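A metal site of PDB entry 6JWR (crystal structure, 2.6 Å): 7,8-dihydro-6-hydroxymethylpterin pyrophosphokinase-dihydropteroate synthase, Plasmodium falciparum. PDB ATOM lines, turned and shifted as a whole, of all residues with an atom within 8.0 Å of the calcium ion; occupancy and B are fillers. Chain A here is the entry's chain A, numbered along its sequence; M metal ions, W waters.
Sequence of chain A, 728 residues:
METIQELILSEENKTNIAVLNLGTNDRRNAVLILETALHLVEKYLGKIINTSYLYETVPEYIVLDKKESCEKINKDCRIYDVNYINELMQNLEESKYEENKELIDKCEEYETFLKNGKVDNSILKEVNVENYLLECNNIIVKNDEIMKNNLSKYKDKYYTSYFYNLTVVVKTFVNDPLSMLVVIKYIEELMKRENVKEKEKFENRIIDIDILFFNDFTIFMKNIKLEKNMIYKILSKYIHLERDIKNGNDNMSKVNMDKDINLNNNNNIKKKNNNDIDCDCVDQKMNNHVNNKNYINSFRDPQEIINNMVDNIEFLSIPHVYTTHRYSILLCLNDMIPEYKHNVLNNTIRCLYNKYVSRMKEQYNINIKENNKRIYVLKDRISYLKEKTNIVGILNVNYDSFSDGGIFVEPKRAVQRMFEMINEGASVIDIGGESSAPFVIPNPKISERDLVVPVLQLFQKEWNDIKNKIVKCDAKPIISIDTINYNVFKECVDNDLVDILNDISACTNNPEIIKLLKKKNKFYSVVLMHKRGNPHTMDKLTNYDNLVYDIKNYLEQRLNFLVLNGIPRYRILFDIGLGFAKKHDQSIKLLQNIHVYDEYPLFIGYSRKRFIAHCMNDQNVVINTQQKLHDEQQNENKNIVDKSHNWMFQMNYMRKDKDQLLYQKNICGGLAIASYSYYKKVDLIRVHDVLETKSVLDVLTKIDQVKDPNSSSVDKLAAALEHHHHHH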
ATOM      1  N   LEU A  38     -12.288   1.898  13.896  1.00  0.00           N
ATOM      2  CA  LEU A  38     -11.945   2.795  12.800  1.00  0.00           C
ATOM      3  C   LEU A  38     -10.455   2.856  12.540  1.00  0.00           C
ATOM      4  O   LEU A  38     -10.045   2.828  11.386  1.00  0.00           O
ATOM      5  CB  LEU A  38     -12.460   4.213  13.062  1.00  0.00           C
ATOM      6  CG  LEU A  38     -13.962   4.422  12.965  1.00  0.00           C
ATOM      7  CD1 LEU A  38     -14.214   5.915  12.891  1.00  0.00           C
ATOM      8  CD2 LEU A  38     -14.511   3.726  11.746  1.00  0.00           C
ATOM      9  N   HIS A  39      -9.657   2.938  13.604  1.00  0.00           N
ATOM     10  CA  HIS A  39      -8.210   2.944  13.433  1.00  0.00           C
ATOM     11  C   HIS A  39      -7.711   1.651  12.817  1.00  0.00           C
ATOM     12  O   HIS A  39      -6.876   1.680  11.910  1.00  0.00           O
ATOM     13  CB  HIS A  39      -7.436   3.266  14.726  1.00  0.00           C
ATOM     14  CG  HIS A  39      -5.946   3.200  14.550  1.00  0.00           C
ATOM     15  ND1 HIS A  39      -5.270   3.944  13.585  1.00  0.00           N
ATOM     16  CD2 HIS A  39      -5.003   2.436  15.152  1.00  0.00           C
ATOM     17  CE1 HIS A  39      -3.977   3.650  13.634  1.00  0.00           C
ATOM     18  NE2 HIS A  39      -3.794   2.751  14.584  1.00  0.00           N
ATOM     19  N   LEU A  40      -8.209   0.517  13.308  1.00  0.00           N
ATOM     20  CA  LEU A  40      -7.797  -0.785  12.777  1.00  0.00           C
ATOM     21  C   LEU A  40      -8.236  -0.983  11.326  1.00  0.00           C
ATOM     22  O   LEU A  40      -7.477  -1.511  10.522  1.00  0.00           O
ATOM     23  CB  LEU A  40      -8.230  -1.935  13.693  1.00  0.00           C
ATOM     24  CG  LEU A  40      -7.642  -1.872  15.132  1.00  0.00           C
ATOM     25  CD1 LEU A  40      -8.366  -2.798  16.097  1.00  0.00           C
ATOM     26  CD2 LEU A  40      -6.143  -2.096  15.187  1.00  0.00           C
ATOM     27  N   VAL A  41      -9.428  -0.496  10.997  1.00  0.00           N
ATOM     28  CA  VAL A  41      -9.927  -0.448   9.633  1.00  0.00           C
ATOM     29  C   VAL A  41      -8.952   0.383   8.783  1.00  0.00           C
ATOM     30  O   VAL A  41      -8.496  -0.087   7.732  1.00  0.00           O
ATOM     31  CB  VAL A  41     -11.360   0.153   9.557  1.00  0.00           C
ATOM     32  CG1 VAL A  41     -11.718   0.611   8.148  1.00  0.00           C
ATOM     33  CG2 VAL A  41     -12.410  -0.838  10.050  1.00  0.00           C
ATOM     34  N   GLU A  42      -8.634   1.602   9.261  1.00  0.00           N
ATOM     35  CA  GLU A  42      -7.753   2.545   8.552  1.00  0.00           C
ATOM     36  C   GLU A  42      -6.372   1.939   8.408  1.00  0.00           C
ATOM     37  O   GLU A  42      -5.723   2.134   7.380  1.00  0.00           O
ATOM     38  CB  GLU A  42      -7.694   3.892   9.283  1.00  0.00           C
ATOM     39  CG  GLU A  42      -6.849   5.005   8.644  1.00  0.00           C
ATOM     40  CD  GLU A  42      -7.374   5.521   7.294  1.00  0.00           C
ATOM     41  OE1 GLU A  42      -8.463   6.140   7.231  1.00  0.00           O
ATOM     42  OE2 GLU A  42      -6.683   5.315   6.279  1.00  0.00           O
ATOM     43  N   LYS A  43      -5.974   1.154   9.409  1.00  0.00           N
ATOM     44  CA  LYS A  43      -4.682   0.464   9.453  1.00  0.00           C
ATOM     45  C   LYS A  43      -4.600  -0.801   8.584  1.00  0.00           C
ATOM     46  O   LYS A  43      -3.635  -0.935   7.828  1.00  0.00           O
ATOM     47  CB  LYS A  43      -4.322   0.117  10.909  1.00  0.00           C
ATOM     48  CG  LYS A  43      -2.954  -0.491  11.147  1.00  0.00           C
ATOM     49  CD  LYS A  43      -2.752  -0.735  12.641  1.00  0.00           C
ATOM     50  CE  LYS A  43      -1.303  -1.112  12.973  1.00  0.00           C
ATOM     51  NZ  LYS A  43      -0.280  -0.113  12.516  1.00  0.00           N
ATOM     52  N   TYR A  44      -5.587  -1.696   8.711  1.00  0.00           N
ATOM     53  CA  TYR A  44      -5.530  -3.034   8.065  1.00  0.00           C
ATOM     54  C   TYR A  44      -6.320  -3.229   6.751  1.00  0.00           C
ATOM     55  O   TYR A  44      -6.106  -4.204   6.028  1.00  0.00           O
ATOM     56  CB  TYR A  44      -5.895  -4.146   9.049  1.00  0.00           C
ATOM     57  CG  TYR A  44      -4.951  -4.297  10.208  1.00  0.00           C
ATOM     58  CD1 TYR A  44      -3.558  -4.333  10.002  1.00  0.00           C
ATOM     59  CD2 TYR A  44      -5.430  -4.448  11.519  1.00  0.00           C
ATOM     60  CE1 TYR A  44      -2.679  -4.481  11.063  1.00  0.00           C
ATOM     61  CE2 TYR A  44      -4.549  -4.601  12.597  1.00  0.00           C
ATOM     62  CZ  TYR A  44      -3.189  -4.618  12.357  1.00  0.00           C
ATOM     63  OH  TYR A  44      -2.306  -4.769  13.405  1.00  0.00           O
ATOM     64  N   LEU A  45      -7.226  -2.307   6.422  1.00  0.00           N
ATOM     65  CA  LEU A  45      -8.119  -2.504   5.276  1.00  0.00           C
ATOM     66  C   LEU A  45      -7.915  -1.542   4.112  1.00  0.00           C
ATOM     67  O   LEU A  45      -8.016  -1.945   2.944  1.00  0.00           O
ATOM     68  CB  LEU A  45      -9.590  -2.544   5.751  1.00  0.00           C
ATOM     69  CG  LEU A  45      -9.959  -3.701   6.714  1.00  0.00           C
ATOM     70  CD1 LEU A  45     -11.310  -3.509   7.365  1.00  0.00           C
ATOM     71  CD2 LEU A  45      -9.922  -5.047   6.005  1.00  0.00           C
ATOM     72  N   GLY A  46      -7.599  -0.298   4.415  1.00  0.00           N
ATOM     73  CA  GLY A  46      -7.418   0.730   3.380  1.00  0.00           C
ATOM     74  C   GLY A  46      -7.688   2.109   3.938  1.00  0.00           C
ATOM     75  O   GLY A  46      -7.310   2.405   5.067  1.00  0.00           O
ATOM     76  N   LYS A  47      -8.372   2.936   3.156  1.00  0.00           N
ATOM     77  CA  LYS A  47      -8.586   4.334   3.494  1.00  0.00           C
ATOM     78  C   LYS A  47     -10.063   4.620   3.772  1.00  0.00           C
ATOM     79  O   LYS A  47     -10.915   4.363   2.921  1.00  0.00           O
ATOM     80  CB  LYS A  47      -8.070   5.229   2.352  1.00  0.00           C
ATOM     81  CG  LYS A  47      -8.082   6.697   2.739  1.00  0.00           C
ATOM     82  CD  LYS A  47      -7.740   7.656   1.617  1.00  0.00           C
ATOM     83  CE  LYS A  47      -7.820   9.088   2.121  1.00  0.00           C
ATOM     84  NZ  LYS A  47      -7.242   9.335   3.485  1.00  0.00           N
ATOM     85  N   ILE A  48     -10.365   5.150   4.959  1.00  0.00           N
ATOM     86  CA  ILE A  48     -11.734   5.561   5.291  1.00  0.00           C
ATOM     87  C   ILE A  48     -12.085   6.831   4.489  1.00  0.00           C
ATOM     88  O   ILE A  48     -11.424   7.864   4.649  1.00  0.00           O
ATOM     89  CB  ILE A  48     -11.916   5.769   6.820  1.00  0.00           C
ATOM     90  CG1 ILE A  48     -11.740   4.433   7.541  1.00  0.00           C
ATOM     91  CG2 ILE A  48     -13.289   6.392   7.147  1.00  0.00           C
ATOM     92  CD1 ILE A  48     -11.766   4.521   9.057  1.00  0.00           C
ATOM     93  N   SER A  95       0.854  -3.235   9.268  1.00  0.00           N
ATOM     94  CA  SER A  95       0.224  -3.540   7.999  1.00  0.00           C
ATOM     95  C   SER A  95       1.315  -3.647   6.965  1.00  0.00           C
ATOM     96  O   SER A  95       2.301  -2.897   7.013  1.00  0.00           O
ATOM     97  CB  SER A  95      -0.761  -2.446   7.604  1.00  0.00           C
ATOM     98  OG  SER A  95      -1.184  -2.566   6.252  1.00  0.00           O
ATOM     99  N   TYR A  97       0.722  -2.757   4.143  1.00  0.00           N
ATOM    100  CA  TYR A  97       0.299  -1.665   3.247  1.00  0.00           C
ATOM    101  C   TYR A  97       0.464  -0.315   3.915  1.00  0.00           C
ATOM    102  O   TYR A  97       0.299  -0.167   5.127  1.00  0.00           O
ATOM    103  CB  TYR A  97      -1.146  -1.862   2.797  1.00  0.00           C
ATOM    104  CG  TYR A  97      -1.319  -2.944   1.758  1.00  0.00           C
ATOM    105  CD1 TYR A  97      -1.375  -4.307   2.139  1.00  0.00           C
ATOM    106  CD2 TYR A  97      -1.449  -2.627   0.400  1.00  0.00           C
ATOM    107  CE1 TYR A  97      -1.524  -5.309   1.193  1.00  0.00           C
ATOM    108  CE2 TYR A  97      -1.615  -3.642  -0.555  1.00  0.00           C
ATOM    109  CZ  TYR A  97      -1.654  -4.971  -0.138  1.00  0.00           C
ATOM    110  OH  TYR A  97      -1.832  -5.988  -1.044  1.00  0.00           O
ATOM    111  N   GLU A  98       0.803   0.677   3.118  1.00  0.00           N
ATOM    112  CA  GLU A  98       1.259   1.922   3.698  1.00  0.00           C
ATOM    113  C   GLU A  98       0.123   2.879   3.907  1.00  0.00           C
ATOM    114  O   GLU A  98      -0.795   2.944   3.097  1.00  0.00           O
ATOM    115  CB  GLU A  98       2.331   2.544   2.808  1.00  0.00           C
ATOM    116  CG  GLU A  98       1.788   3.092   1.514  1.00  0.00           C
ATOM    117  CD  GLU A  98       2.622   2.679   0.351  1.00  0.00           C
ATOM    118  OE1 GLU A  98       2.018   2.293  -0.666  1.00  0.00           O
ATOM    119  OE2 GLU A  98       3.867   2.734   0.492  1.00  0.00           O
ATOM    120  N   GLU A  99       0.180   3.635   4.989  1.00  0.00           N
ATOM    121  CA  GLU A  99      -0.789   4.692   5.182  1.00  0.00           C
ATOM    122  C   GLU A  99      -0.348   5.934   4.427  1.00  0.00           C
ATOM    123  O   GLU A  99       0.829   6.262   4.389  1.00  0.00           O
ATOM    124  CB  GLU A  99      -1.021   4.995   6.651  1.00  0.00           C
ATOM    125  CG  GLU A  99      -2.405   5.560   6.890  1.00  0.00           C
ATOM    126  CD  GLU A  99      -3.121   4.839   7.996  1.00  0.00           C
ATOM    127  OE1 GLU A  99      -3.465   3.670   7.753  1.00  0.00           O
ATOM    128  OE2 GLU A  99      -3.349   5.403   9.091  1.00  0.00           O
ATOM    129  N   ASN A 100      -1.286   6.616   3.783  1.00  0.00           N
ATOM    130  CA  ASN A 100      -0.991   7.888   3.187  1.00  0.00           C
ATOM    131  C   ASN A 100      -1.972   8.903   3.748  1.00  0.00           C
ATOM    132  O   ASN A 100      -3.176   8.774   3.564  1.00  0.00           O
ATOM    133  CB  ASN A 100      -0.982   7.801   1.667  1.00  0.00           C
ATOM    134  CG  ASN A 100      -0.012   6.742   1.142  1.00  0.00           C
ATOM    135  OD1 ASN A 100      -0.358   5.941   0.273  1.00  0.00           O
ATOM    136  ND2 ASN A 100       1.209   6.713   1.686  1.00  0.00           N
ATOM    137  N   LYS A 101      -1.448   9.879   4.478  1.00  0.00           N
ATOM    138  CA  LYS A 101      -2.272  10.883   5.100  1.00  0.00           C
ATOM    139  C   LYS A 101      -2.480  12.125   4.219  1.00  0.00           C
ATOM    140  O   LYS A 101      -3.234  13.007   4.601  1.00  0.00           O
ATOM    141  CB  LYS A 101      -1.712  11.268   6.478  1.00  0.00           C
ATOM    142  CG  LYS A 101      -1.723  10.170   7.552  1.00  0.00           C
ATOM    143  CD  LYS A 101      -1.359  10.710   8.941  1.00  0.00           C
ATOM    144  CE  LYS A 101      -2.572  11.357   9.613  1.00  0.00           C
ATOM    145  NZ  LYS A 101      -2.325  11.906  10.972  1.00  0.00           N
ATOM    146  N   VAL A 170     -14.810   2.307   3.009  1.00  0.00           N
ATOM    147  CA  VAL A 170     -13.368   2.132   2.946  1.00  0.00           C
ATOM    148  C   VAL A 170     -12.959   1.947   1.496  1.00  0.00           C
ATOM    149  O   VAL A 170     -13.537   1.120   0.806  1.00  0.00           O
ATOM    150  CB  VAL A 170     -12.875   0.904   3.744  1.00  0.00           C
ATOM    151  CG1 VAL A 170     -11.360   1.005   3.963  1.00  0.00           C
ATOM    152  CG2 VAL A 170     -13.601   0.787   5.072  1.00  0.00           C
ATOM    153  N   LYS A 171     -11.972   2.715   1.053  1.00  0.00           N
ATOM    154  CA  LYS A 171     -11.288   2.434  -0.215  1.00  0.00           C
ATOM    155  C   LYS A 171     -10.205   1.376   0.085  1.00  0.00           C
ATOM    156  O   LYS A 171      -9.160   1.682   0.685  1.00  0.00           O
ATOM    157  CB  LYS A 171     -10.692   3.721  -0.771  1.00  0.00           C
ATOM    158  CG  LYS A 171     -10.067   3.658  -2.147  1.00  0.00           C
ATOM    159  CD  LYS A 171      -9.115   4.845  -2.272  1.00  0.00           C
ATOM    160  CE  LYS A 171      -9.135   5.466  -3.655  1.00  0.00           C
ATOM    161  NZ  LYS A 171      -8.905   6.934  -3.541  1.00  0.00           N
ATOM    162  N   PHE A 173      -7.612  -2.112  -0.300  1.00  0.00           N
ATOM    163  CA  PHE A 173      -6.587  -2.848  -1.029  1.00  0.00           C
ATOM    164  C   PHE A 173      -6.764  -4.354  -0.842  1.00  0.00           C
ATOM    165  O   PHE A 173      -5.967  -5.132  -1.344  1.00  0.00           O
ATOM    166  CB  PHE A 173      -5.165  -2.436  -0.574  1.00  0.00           C
ATOM    167  CG  PHE A 173      -4.983  -2.400   0.935  1.00  0.00           C
ATOM    168  CD1 PHE A 173      -5.075  -3.562   1.698  1.00  0.00           C
ATOM    169  CD2 PHE A 173      -4.676  -1.201   1.592  1.00  0.00           C
ATOM    170  CE1 PHE A 173      -4.915  -3.520   3.083  1.00  0.00           C
ATOM    171  CE2 PHE A 173      -4.501  -1.154   2.964  1.00  0.00           C
ATOM    172  CZ  PHE A 173      -4.614  -2.320   3.716  1.00  0.00           C
ATOM    173  N   LYS A 518      -6.488  13.501  13.268  1.00  0.00           N
ATOM    174  CA  LYS A 518      -6.333  12.049  13.451  1.00  0.00           C
ATOM    175  C   LYS A 518      -4.973  11.744  14.081  1.00  0.00           C
ATOM    176  O   LYS A 518      -3.949  12.164  13.566  1.00  0.00           O
ATOM    177  CB  LYS A 518      -6.445  11.299  12.118  1.00  0.00           C
ATOM    178  CG  LYS A 518      -7.530  11.768  11.153  1.00  0.00           C
ATOM    179  CD  LYS A 518      -6.992  11.875   9.716  1.00  0.00           C
ATOM    180  CE  LYS A 518      -7.560  10.820   8.783  1.00  0.00           C
ATOM    181  NZ  LYS A 518      -7.816   9.502   9.426  1.00  0.00           N
HETATM  182 CA    CA M   1      -5.027   3.537   5.731  1.00  0.00          CA
HETATM  183  O   HOH W   1      -5.118   3.812   3.592  1.00  0.00           O
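The backbone NH (N) of Ile 48 sits at hydrogen-bond distance from the side-chain carboxylate (OE1) of Glu 42. O of Val 41 is in hydrogen-bond range of N of Gly 46.
The nearest printed residue that does not touch the calcium ion is Lys 47 (4.3 Å).
The calcium ion is bound by water W1, O of Glu 42, OE2 of Glu 42, OE1 of Glu 99 and O of Gly 46.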
